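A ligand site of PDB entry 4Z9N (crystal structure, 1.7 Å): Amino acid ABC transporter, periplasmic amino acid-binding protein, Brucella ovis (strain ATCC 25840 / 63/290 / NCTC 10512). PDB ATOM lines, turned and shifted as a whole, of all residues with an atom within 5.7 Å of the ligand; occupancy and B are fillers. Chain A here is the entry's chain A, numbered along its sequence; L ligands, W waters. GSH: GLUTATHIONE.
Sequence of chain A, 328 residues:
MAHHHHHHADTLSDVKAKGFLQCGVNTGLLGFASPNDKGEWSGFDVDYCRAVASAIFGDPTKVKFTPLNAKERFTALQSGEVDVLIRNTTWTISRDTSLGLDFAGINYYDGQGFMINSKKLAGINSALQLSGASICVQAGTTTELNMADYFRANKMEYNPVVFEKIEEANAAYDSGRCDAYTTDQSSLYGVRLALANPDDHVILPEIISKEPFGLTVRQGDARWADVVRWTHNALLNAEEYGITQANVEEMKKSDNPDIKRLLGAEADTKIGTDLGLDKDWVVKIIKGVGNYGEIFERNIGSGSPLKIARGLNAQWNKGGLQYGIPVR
OG1 of Thr 27 is in hydrogen-bond range of O32 of the ligand.
The side-chain carboxylate (OD2) of Asp 184 is in salt-bridge range of a nitrogen (N1) of the ligand (2.6 Å).
An oxygen (O2) of the ligand sits at hydrogen-bond distance from the side-chain amide nitrogen of Asn 26, 2.8 Å away.
O11 of the ligand lies within salt-bridge range of NH1 of Arg 95 (2.8 Å).
An oxygen (O31) of the ligand sits at hydrogen-bond distance from the side-chain amide nitrogen of Gln 138.
N of Thr 90 is in hydrogen-bond range of O11 of the ligand (2.9 Å).
The side-chain hydroxyl (OG1) of Thr 90 is in hydrogen-bond range of a nitrogen (N1) of the ligand.
O of Asn 88 lies within hydrogen-bond range of N1 of the ligand (3.0 Å).
O2 of the ligand is in hydrogen-bond range of ND2 of Asn 88.
The guanidinium group (NH2) of Arg 73 is in salt-bridge range of an oxygen (O12) of the ligand (2.9 Å).
An oxygen (O12) of the ligand lies within hydrogen-bond range of the backbone NH (N) of Thr 142, 3.0 Å away.
The side-chain hydroxyl (OG1) of Thr 142 is in hydrogen-bond range of an oxygen (O12) of the ligand, at 3.3 Å.
The backbone NH (N) of Ala 70 is in hydrogen-bond range of an oxygen (O31) of the ligand, at 3.0 Å.
The guanidinium group (NH2) of Arg 87 lies within salt-bridge range of an oxygen (O31) of the ligand, 3.0 Å away.
The side-chain hydroxyl of Thr 183 lies close to a sulfur (SG2) of the ligand (3.5 Å).
The side-chain hydroxyl (OG) of Ser 187 sits close to a sulfur (SG2) of the ligand (3.7 Å).
A nitrogen (N1) of the ligand lies within salt-bridge range of the side-chain carboxylate of Glu 211.
Water W3 lies within hydrogen-bond range of an oxygen (O32) of the ligand (2.7 Å) and the backbone NH of Ile 166 (2.9 Å).
Water W2 lies within hydrogen-bond range of the side-chain carboxylate (OD2) of Asp 184, the side-chain hydroxyl (OG) of Ser 187, the side-chain amide nitrogen (ND2) of Asn 88, a nitrogen (N2) of the ligand and the side-chain hydroxyl (OG1) of Thr 183.
Water W4 lies within hydrogen-bond range of OG1 of Thr 143 (2.7 Å), OG1 of Thr 183 (2.8 Å) and N2 of the ligand (3.3 Å).
Water W1 bridges the side-chain amide oxygen of Gln 138 and the side-chain hydroxyl of Tyr 181.
The side-chain amide oxygen of Asn 26 is in hydrogen-bond range of the backbone NH of Gly 28.
NH1 of Arg 95 sits at hydrogen-bond distance from O of Thr 90.
The side-chain hydroxyl (OG1) of Thr 90 sits at hydrogen-bond distance from the side-chain carboxylate (OE1) of Glu 211 (2.6 Å).
The guanidinium group (NH1) of Arg 73 sits at hydrogen-bond distance from the side-chain hydroxyl (OG1) of Thr 89.
The backbone carbonyl oxygen (O) of Gly 140 lies within hydrogen-bond range of the guanidinium group (NH2) of Arg 73.
OG1 of Thr 142 lies within hydrogen-bond range of OE1 of Glu 211.
The side-chain hydroxyl of Thr 89 lies within hydrogen-bond range of the backbone carbonyl oxygen of Arg 87 (2.7 Å).
OG1 of Thr 141 lies close to N of Thr 143 (3.4 Å).
Merely in contact with the ligand: Thr 141, Asn 69, Thr 89, Ile 166, Thr 143, Phe 213 and Leu 68.
Hydrophobic or aromatic side chains within 4 Å of the ligand: Ala 70, Ile 166 and Phe 213.
Of the 29 residues printed, 21 come within 4 Å of the ligand.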
ATOM      1  N   ASN A  26     -26.534 -35.426  16.869  1.00  0.00           N
ATOM      2  CA  ASN A  26     -27.754 -34.682  16.527  1.00  0.00           C
ATOM      3  C   ASN A  26     -28.819 -34.779  17.623  1.00  0.00           C
ATOM      4  O   ASN A  26     -28.787 -35.685  18.444  1.00  0.00           O
ATOM      5  CB  ASN A  26     -28.310 -35.224  15.209  1.00  0.00           C
ATOM      6  CG  ASN A  26     -29.127 -34.217  14.469  1.00  0.00           C
ATOM      7  OD1 ASN A  26     -30.278 -33.965  14.824  1.00  0.00           O
ATOM      8  ND2 ASN A  26     -28.558 -33.639  13.402  1.00  0.00           N
ATOM      9  N   THR A  27     -29.771 -33.840  17.653  1.00  0.00           N
ATOM     10  CA  THR A  27     -30.921 -33.988  18.558  1.00  0.00           C
ATOM     11  C   THR A  27     -31.912 -35.043  18.073  1.00  0.00           C
ATOM     12  O   THR A  27     -32.680 -35.613  18.865  1.00  0.00           O
ATOM     13  CB  THR A  27     -31.676 -32.656  18.741  1.00  0.00           C
ATOM     14  OG1 THR A  27     -32.155 -32.180  17.469  1.00  0.00           O
ATOM     15  CG2 THR A  27     -30.779 -31.618  19.398  1.00  0.00           C
ATOM     16  N   GLY A  28     -31.913 -35.305  16.775  1.00  0.00           N
ATOM     17  CA  GLY A  28     -32.832 -36.284  16.212  1.00  0.00           C
ATOM     18  C   GLY A  28     -32.987 -36.144  14.714  1.00  0.00           C
ATOM     19  O   GLY A  28     -33.726 -35.292  14.220  1.00  0.00           O
ATOM     20  N   LEU A  29     -32.259 -36.969  13.988  1.00  0.00           N
ATOM     21  CA  LEU A  29     -32.282 -36.930  12.533  1.00  0.00           C
ATOM     22  C   LEU A  29     -32.216 -38.367  12.069  1.00  0.00           C
ATOM     23  O   LEU A  29     -31.192 -39.033  12.248  1.00  0.00           O
ATOM     24  CB  LEU A  29     -31.099 -36.129  11.982  1.00  0.00           C
ATOM     25  CG  LEU A  29     -30.986 -36.084  10.449  1.00  0.00           C
ATOM     26  CD1 LEU A  29     -32.231 -35.413   9.830  1.00  0.00           C
ATOM     27  CD2 LEU A  29     -29.698 -35.377  10.026  1.00  0.00           C
ATOM     28  N   LEU A  68     -27.040 -32.221  20.458  1.00  0.00           N
ATOM     29  CA  LEU A  68     -26.714 -30.796  20.297  1.00  0.00           C
ATOM     30  C   LEU A  68     -27.423 -30.199  19.102  1.00  0.00           C
ATOM     31  O   LEU A  68     -27.427 -30.792  18.020  1.00  0.00           O
ATOM     32  CB  LEU A  68     -25.204 -30.621  20.116  1.00  0.00           C
ATOM     33  CG  LEU A  68     -24.356 -31.202  21.242  1.00  0.00           C
ATOM     34  CD1 LEU A  68     -22.899 -31.338  20.784  1.00  0.00           C
ATOM     35  CD2 LEU A  68     -24.496 -30.307  22.467  1.00  0.00           C
ATOM     36  N   ASN A  69     -27.993 -29.004  19.260  1.00  0.00           N
ATOM     37  CA  ASN A  69     -28.593 -28.380  18.089  1.00  0.00           C
ATOM     38  C   ASN A  69     -27.535 -27.607  17.298  1.00  0.00           C
ATOM     39  O   ASN A  69     -26.359 -27.567  17.674  1.00  0.00           O
ATOM     40  CB  ASN A  69     -29.785 -27.474  18.487  1.00  0.00           C
ATOM     41  CG  ASN A  69     -29.381 -26.286  19.340  1.00  0.00           C
ATOM     42  OD1 ASN A  69     -28.273 -25.744  19.234  1.00  0.00           O
ATOM     43  ND2 ASN A  69     -30.321 -25.828  20.187  1.00  0.00           N
ATOM     44  N   ALA A  70     -27.957 -26.971  16.210  1.00  0.00           N
ATOM     45  CA  ALA A  70     -27.002 -26.377  15.302  1.00  0.00           C
ATOM     46  C   ALA A  70     -26.240 -25.218  15.941  1.00  0.00           C
ATOM     47  O   ALA A  70     -25.092 -24.968  15.565  1.00  0.00           O
ATOM     48  CB  ALA A  70     -27.703 -25.913  14.016  1.00  0.00           C
ATOM     49  N   LYS A  71     -26.859 -24.539  16.908  1.00  0.00           N
ATOM     50  CA  LYS A  71     -26.248 -23.376  17.532  1.00  0.00           C
ATOM     51  C   LYS A  71     -25.271 -23.734  18.655  1.00  0.00           C
ATOM     52  O   LYS A  71     -24.295 -23.034  18.859  1.00  0.00           O
ATOM     53  CB  LYS A  71     -27.329 -22.415  18.081  1.00  0.00           C
ATOM     54  N   ARG A  73     -23.599 -26.775  19.101  1.00  0.00           N
ATOM     55  CA  ARG A  73     -22.692 -27.901  18.820  1.00  0.00           C
ATOM     56  C   ARG A  73     -21.191 -27.563  18.970  1.00  0.00           C
ATOM     57  O   ARG A  73     -20.421 -28.375  19.493  1.00  0.00           O
ATOM     58  CB  ARG A  73     -22.953 -28.433  17.412  1.00  0.00           C
ATOM     59  CG  ARG A  73     -22.866 -27.386  16.325  1.00  0.00           C
ATOM     60  CD  ARG A  73     -23.159 -27.975  14.964  1.00  0.00           C
ATOM     61  NE  ARG A  73     -23.720 -26.974  14.071  1.00  0.00           N
ATOM     62  CZ  ARG A  73     -23.711 -27.062  12.742  1.00  0.00           C
ATOM     63  NH1 ARG A  73     -23.150 -28.114  12.146  1.00  0.00           N
ATOM     64  NH2 ARG A  73     -24.270 -26.102  12.008  1.00  0.00           N
ATOM     65  N   PHE A  74     -20.764 -26.391  18.520  1.00  0.00           N
ATOM     66  CA  PHE A  74     -19.335 -26.081  18.547  1.00  0.00           C
ATOM     67  C   PHE A  74     -18.869 -25.750  19.958  1.00  0.00           C
ATOM     68  O   PHE A  74     -17.788 -26.165  20.377  1.00  0.00           O
ATOM     69  CB  PHE A  74     -19.007 -24.956  17.569  1.00  0.00           C
ATOM     70  CG  PHE A  74     -19.314 -25.299  16.144  1.00  0.00           C
ATOM     71  CD1 PHE A  74     -18.586 -26.304  15.484  1.00  0.00           C
ATOM     72  CD2 PHE A  74     -20.340 -24.676  15.472  1.00  0.00           C
ATOM     73  CE1 PHE A  74     -18.906 -26.652  14.172  1.00  0.00           C
ATOM     74  CE2 PHE A  74     -20.642 -25.011  14.148  1.00  0.00           C
ATOM     75  CZ  PHE A  74     -19.913 -26.001  13.505  1.00  0.00           C
ATOM     76  N   ARG A  87     -21.706 -35.149  13.715  1.00  0.00           N
ATOM     77  CA  ARG A  87     -23.062 -34.614  13.715  1.00  0.00           C
ATOM     78  C   ARG A  87     -23.311 -33.792  12.462  1.00  0.00           C
ATOM     79  O   ARG A  87     -23.538 -32.594  12.546  1.00  0.00           O
ATOM     80  CB  ARG A  87     -23.280 -33.778  14.992  1.00  0.00           C
ATOM     81  CG  ARG A  87     -24.700 -33.196  15.188  1.00  0.00           C
ATOM     82  CD  ARG A  87     -24.591 -31.737  15.635  1.00  0.00           C
ATOM     83  NE  ARG A  87     -25.861 -31.016  15.594  1.00  0.00           N
ATOM     84  CZ  ARG A  87     -26.356 -30.470  14.489  1.00  0.00           C
ATOM     85  NH1 ARG A  87     -25.697 -30.604  13.338  1.00  0.00           N
ATOM     86  NH2 ARG A  87     -27.491 -29.803  14.526  1.00  0.00           N
ATOM     87  N   ASN A  88     -23.270 -34.450  11.316  1.00  0.00           N
ATOM     88  CA  ASN A  88     -23.575 -33.844  10.008  1.00  0.00           C
ATOM     89  C   ASN A  88     -23.076 -32.393   9.916  1.00  0.00           C
ATOM     90  O   ASN A  88     -23.797 -31.490   9.502  1.00  0.00           O
ATOM     91  CB  ASN A  88     -25.092 -33.964   9.667  1.00  0.00           C
ATOM     92  CG  ASN A  88     -26.031 -33.470  10.777  1.00  0.00           C
ATOM     93  OD1 ASN A  88     -26.084 -34.046  11.871  1.00  0.00           O
ATOM     94  ND2 ASN A  88     -26.831 -32.453  10.468  1.00  0.00           N
ATOM     95  N   THR A  89     -21.822 -32.198  10.347  1.00  0.00           N
ATOM     96  CA  THR A  89     -21.249 -30.867  10.464  1.00  0.00           C
ATOM     97  C   THR A  89     -20.212 -30.600   9.384  1.00  0.00           C
ATOM     98  O   THR A  89     -19.211 -31.308   9.305  1.00  0.00           O
ATOM     99  CB  THR A  89     -20.621 -30.655  11.866  1.00  0.00           C
ATOM    100  OG1 THR A  89     -21.680 -30.610  12.833  1.00  0.00           O
ATOM    101  CG2 THR A  89     -19.809 -29.343  11.921  1.00  0.00           C
ATOM    102  N   THR A  90     -20.451 -29.577   8.576  1.00  0.00           N
ATOM    103  CA  THR A  90     -19.632 -29.311   7.399  1.00  0.00           C
ATOM    104  C   THR A  90     -18.279 -28.722   7.763  1.00  0.00           C
ATOM    105  O   THR A  90     -18.212 -27.805   8.559  1.00  0.00           O
ATOM    106  CB  THR A  90     -20.345 -28.373   6.432  1.00  0.00           C
ATOM    107  OG1 THR A  90     -21.586 -28.967   6.036  1.00  0.00           O
ATOM    108  CG2 THR A  90     -19.483 -28.106   5.185  1.00  0.00           C
ATOM    109  N   ARG A  95     -14.576 -22.565  10.051  1.00  0.00           N
ATOM    110  CA  ARG A  95     -14.680 -23.473  11.194  1.00  0.00           C
ATOM    111  C   ARG A  95     -13.327 -24.120  11.515  1.00  0.00           C
ATOM    112  O   ARG A  95     -13.079 -24.542  12.647  1.00  0.00           O
ATOM    113  CB  ARG A  95     -15.739 -24.544  10.932  1.00  0.00           C
ATOM    114  CG  ARG A  95     -17.136 -23.955  10.759  1.00  0.00           C
ATOM    115  CD  ARG A  95     -18.140 -24.995  10.296  1.00  0.00           C
ATOM    116  NE  ARG A  95     -19.495 -24.447  10.326  1.00  0.00           N
ATOM    117  CZ  ARG A  95     -20.590 -25.138  10.018  1.00  0.00           C
ATOM    118  NH1 ARG A  95     -20.505 -26.401   9.630  1.00  0.00           N
ATOM    119  NH2 ARG A  95     -21.784 -24.559  10.096  1.00  0.00           N
ATOM    120  N   GLN A 138     -32.403 -23.572   9.280  1.00  0.00           N
ATOM    121  CA  GLN A 138     -31.986 -23.348  10.658  1.00  0.00           C
ATOM    122  C   GLN A 138     -30.881 -22.323  10.766  1.00  0.00           C
ATOM    123  O   GLN A 138     -30.004 -22.259   9.920  1.00  0.00           O
ATOM    124  CB  GLN A 138     -31.515 -24.660  11.293  1.00  0.00           C
ATOM    125  CG  GLN A 138     -32.614 -25.368  12.033  1.00  0.00           C
ATOM    126  CD  GLN A 138     -32.130 -26.613  12.722  1.00  0.00           C
ATOM    127  OE1 GLN A 138     -32.202 -27.699  12.152  1.00  0.00           O
ATOM    128  NE2 GLN A 138     -31.638 -26.467  13.943  1.00  0.00           N
ATOM    129  N   GLY A 140     -27.438 -20.737  12.380  1.00  0.00           N
ATOM    130  CA  GLY A 140     -26.178 -21.341  12.781  1.00  0.00           C
ATOM    131  C   GLY A 140     -25.717 -22.446  11.857  1.00  0.00           C
ATOM    132  O   GLY A 140     -25.005 -23.354  12.270  1.00  0.00           O
ATOM    133  N   THR A 141     -26.098 -22.349  10.585  1.00  0.00           N
ATOM    134  CA  THR A 141     -25.719 -23.354   9.592  1.00  0.00           C
ATOM    135  C   THR A 141     -25.042 -22.746   8.378  1.00  0.00           C
ATOM    136  O   THR A 141     -25.225 -21.552   8.071  1.00  0.00           O
ATOM    137  CB  THR A 141     -26.952 -24.160   9.081  1.00  0.00           C
ATOM    138  OG1 THR A 141     -27.900 -23.247   8.505  1.00  0.00           O
ATOM    139  CG2 THR A 141     -27.610 -24.944  10.212  1.00  0.00           C
ATOM    140  N   THR A 142     -24.254 -23.564   7.678  1.00  0.00           N
ATOM    141  CA  THR A 142     -23.817 -23.196   6.331  1.00  0.00           C
ATOM    142  C   THR A 142     -25.021 -22.979   5.433  1.00  0.00           C
ATOM    143  O   THR A 142     -25.019 -22.133   4.526  1.00  0.00           O
ATOM    144  CB  THR A 142     -22.924 -24.299   5.716  1.00  0.00           C
ATOM    145  OG1 THR A 142     -23.602 -25.561   5.826  1.00  0.00           O
ATOM    146  CG2 THR A 142     -21.596 -24.367   6.449  1.00  0.00           C
ATOM    147  N   THR A 143     -26.053 -23.773   5.692  1.00  0.00           N
ATOM    148  CA  THR A 143     -27.271 -23.836   4.868  1.00  0.00           C
ATOM    149  C   THR A 143     -27.897 -22.459   4.671  1.00  0.00           C
ATOM    150  O   THR A 143     -28.299 -22.097   3.564  1.00  0.00           O
ATOM    151  CB  THR A 143     -28.284 -24.781   5.535  1.00  0.00           C
ATOM    152  OG1 THR A 143     -27.599 -25.968   5.949  1.00  0.00           O
ATOM    153  CG2 THR A 143     -29.473 -25.134   4.591  1.00  0.00           C
ATOM    154  N   GLU A 164     -34.599 -22.114  15.230  1.00  0.00           N
ATOM    155  CA  GLU A 164     -33.539 -22.601  16.102  1.00  0.00           C
ATOM    156  C   GLU A 164     -33.696 -24.079  16.436  1.00  0.00           C
ATOM    157  O   GLU A 164     -32.733 -24.732  16.835  1.00  0.00           O
ATOM    158  CB  GLU A 164     -33.484 -21.781  17.398  1.00  0.00           C
ATOM    159  CG  GLU A 164     -33.038 -20.357  17.207  1.00  0.00           C
ATOM    160  CD  GLU A 164     -32.547 -19.736  18.504  1.00  0.00           C
ATOM    161  OE1 GLU A 164     -32.214 -20.491  19.456  1.00  0.00           O
ATOM    162  OE2 GLU A 164     -32.498 -18.492  18.581  1.00  0.00           O
ATOM    163  N   ILE A 166     -35.005 -27.923  15.077  1.00  0.00           N
ATOM    164  CA  ILE A 166     -35.364 -28.660  13.884  1.00  0.00           C
ATOM    165  C   ILE A 166     -36.851 -29.085  13.916  1.00  0.00           C
ATOM    166  O   ILE A 166     -37.502 -29.097  12.878  1.00  0.00           O
ATOM    167  CB  ILE A 166     -34.434 -29.903  13.666  1.00  0.00           C
ATOM    168  CG1 ILE A 166     -34.659 -30.482  12.282  1.00  0.00           C
ATOM    169  CG2 ILE A 166     -34.608 -30.959  14.755  1.00  0.00           C
ATOM    170  CD1 ILE A 166     -33.661 -31.558  11.884  1.00  0.00           C
ATOM    171  N   TYR A 181     -38.184 -26.776   2.132  1.00  0.00           N
ATOM    172  CA  TYR A 181     -37.265 -27.068   3.233  1.00  0.00           C
ATOM    173  C   TYR A 181     -35.865 -27.088   2.631  1.00  0.00           C
ATOM    174  O   TYR A 181     -35.683 -27.707   1.570  1.00  0.00           O
ATOM    175  CB  TYR A 181     -37.595 -28.431   3.847  1.00  0.00           C
ATOM    176  CG  TYR A 181     -37.029 -28.696   5.219  1.00  0.00           C
ATOM    177  CD1 TYR A 181     -35.662 -28.830   5.429  1.00  0.00           C
ATOM    178  CD2 TYR A 181     -37.875 -28.868   6.294  1.00  0.00           C
ATOM    179  CE1 TYR A 181     -35.156 -29.081   6.671  1.00  0.00           C
ATOM    180  CE2 TYR A 181     -37.385 -29.114   7.550  1.00  0.00           C
ATOM    181  CZ  TYR A 181     -36.024 -29.232   7.734  1.00  0.00           C
ATOM    182  OH  TYR A 181     -35.531 -29.485   8.997  1.00  0.00           O
ATOM    183  N   THR A 183     -31.742 -28.036   3.490  1.00  0.00           N
ATOM    184  CA  THR A 183     -30.630 -28.520   4.308  1.00  0.00           C
ATOM    185  C   THR A 183     -29.819 -29.474   3.410  1.00  0.00           C
ATOM    186  O   THR A 183     -30.033 -29.541   2.201  1.00  0.00           O
ATOM    187  CB  THR A 183     -31.098 -29.229   5.604  1.00  0.00           C
ATOM    188  OG1 THR A 183     -29.977 -29.621   6.393  1.00  0.00           O
ATOM    189  CG2 THR A 183     -32.001 -30.442   5.294  1.00  0.00           C
ATOM    190  N   ASP A 184     -28.899 -30.201   4.018  1.00  0.00           N
ATOM    191  CA  ASP A 184     -28.113 -31.187   3.272  1.00  0.00           C
ATOM    192  C   ASP A 184     -28.999 -32.285   2.700  1.00  0.00           C
ATOM    193  O   ASP A 184     -29.971 -32.688   3.356  1.00  0.00           O
ATOM    194  CB  ASP A 184     -27.061 -31.774   4.194  1.00  0.00           C
ATOM    195  CG  ASP A 184     -26.159 -30.711   4.797  1.00  0.00           C
ATOM    196  OD1 ASP A 184     -25.746 -29.807   4.035  1.00  0.00           O
ATOM    197  OD2 ASP A 184     -25.922 -30.747   6.021  1.00  0.00           O
ATOM    198  N   SER A 187     -29.862 -35.207   4.798  1.00  0.00           N
ATOM    199  CA  SER A 187     -30.756 -34.809   5.889  1.00  0.00           C
ATOM    200  C   SER A 187     -32.196 -34.702   5.399  1.00  0.00           C
ATOM    201  O   SER A 187     -33.123 -35.039   6.138  1.00  0.00           O
ATOM    202  CB  SER A 187     -30.324 -33.469   6.501  1.00  0.00           C
ATOM    203  OG  SER A 187     -28.959 -33.514   6.859  1.00  0.00           O
ATOM    204  N   VAL A 191     -35.429 -36.110   7.220  1.00  0.00           N
ATOM    205  CA  VAL A 191     -36.535 -35.225   7.584  1.00  0.00           C
ATOM    206  C   VAL A 191     -37.819 -35.726   6.950  1.00  0.00           C
ATOM    207  O   VAL A 191     -38.839 -35.820   7.612  1.00  0.00           O
ATOM    208  CB  VAL A 191     -36.234 -33.778   7.174  1.00  0.00           C
ATOM    209  CG1 VAL A 191     -37.511 -32.923   7.225  1.00  0.00           C
ATOM    210  CG2 VAL A 191     -35.173 -33.193   8.096  1.00  0.00           C
ATOM    211  N   GLU A 211     -20.858 -29.873   1.020  1.00  0.00           N
ATOM    212  CA  GLU A 211     -21.051 -30.019   2.462  1.00  0.00           C
ATOM    213  C   GLU A 211     -20.348 -31.292   2.929  1.00  0.00           C
ATOM    214  O   GLU A 211     -21.007 -32.312   3.175  1.00  0.00           O
ATOM    215  CB  GLU A 211     -22.549 -30.078   2.833  1.00  0.00           C
ATOM    216  CG  GLU A 211     -23.442 -28.937   2.265  1.00  0.00           C
ATOM    217  CD  GLU A 211     -23.392 -27.618   3.047  1.00  0.00           C
ATOM    218  OE1 GLU A 211     -22.769 -27.531   4.151  1.00  0.00           O
ATOM    219  OE2 GLU A 211     -23.965 -26.625   2.532  1.00  0.00           O
ATOM    220  N   PHE A 213     -19.209 -33.588   5.488  1.00  0.00           N
ATOM    221  CA  PHE A 213     -19.411 -33.781   6.930  1.00  0.00           C
ATOM    222  C   PHE A 213     -18.106 -34.198   7.582  1.00  0.00           C
ATOM    223  O   PHE A 213     -17.513 -35.215   7.201  1.00  0.00           O
ATOM    224  CB  PHE A 213     -20.452 -34.870   7.210  1.00  0.00           C
ATOM    225  CG  PHE A 213     -21.860 -34.531   6.792  1.00  0.00           C
ATOM    226  CD1 PHE A 213     -22.202 -33.263   6.329  1.00  0.00           C
ATOM    227  CD2 PHE A 213     -22.851 -35.494   6.857  1.00  0.00           C
ATOM    228  CE1 PHE A 213     -23.510 -32.982   5.922  1.00  0.00           C
ATOM    229  CE2 PHE A 213     -24.153 -35.229   6.476  1.00  0.00           C
ATOM    230  CZ  PHE A 213     -24.492 -33.966   6.006  1.00  0.00           C
HETATM  231  N1  GSH L   1     -24.122 -29.431   7.395  1.00  0.00           N
HETATM  232  CA1 GSH L   1     -24.750 -28.145   7.764  1.00  0.00           C
HETATM  233  C1  GSH L   1     -23.846 -27.377   8.732  1.00  0.00           C
HETATM  234  O11 GSH L   1     -22.811 -27.946   9.190  1.00  0.00           O
HETATM  235  O12 GSH L   1     -24.119 -26.177   9.065  1.00  0.00           O
HETATM  236  CB1 GSH L   1     -26.098 -28.358   8.442  1.00  0.00           C
HETATM  237  CG1 GSH L   1     -25.938 -29.045   9.796  1.00  0.00           C
HETATM  238  CD1 GSH L   1     -27.259 -29.022  10.566  1.00  0.00           C
HETATM  239  OE1 GSH L   1     -27.323 -28.647  11.691  1.00  0.00           O
HETATM  240  N2  GSH L   1     -28.470 -29.490   9.933  1.00  0.00           N
HETATM  241  CA2 GSH L   1     -29.694 -29.396  10.720  1.00  0.00           C
HETATM  242  C2  GSH L   1     -29.720 -30.316  11.937  1.00  0.00           C
HETATM  243  O2  GSH L   1     -29.032 -31.266  12.028  1.00  0.00           O
HETATM  244  CB2 GSH L   1     -30.865 -29.682   9.793  1.00  0.00           C
HETATM  245  SG2 GSH L   1     -30.940 -31.394   9.218  1.00  0.00           S
HETATM  246  N3  GSH L   1     -30.611 -29.981  13.019  1.00  0.00           N
HETATM  247  CA3 GSH L   1     -30.716 -30.794  14.204  1.00  0.00           C
HETATM  248  C3  GSH L   1     -30.644 -29.809  15.361  1.00  0.00           C
HETATM  249  O31 GSH L   1     -30.182 -28.654  15.160  1.00  0.00           O
HETATM  250  O32 GSH L   1     -31.031 -30.173  16.497  1.00  0.00           O
HETATM  251  O   HOH W   1     -33.516 -27.515   9.633  1.00  0.00           O
HETATM  252  O   HOH W   2     -27.538 -31.413   7.928  1.00  0.00           O
HETATM  253  O   HOH W   3     -33.038 -28.495  17.129  1.00  0.00           O
HETATM  254  O   HOH W   4     -29.309 -27.256   7.646  1.00  0.00           O
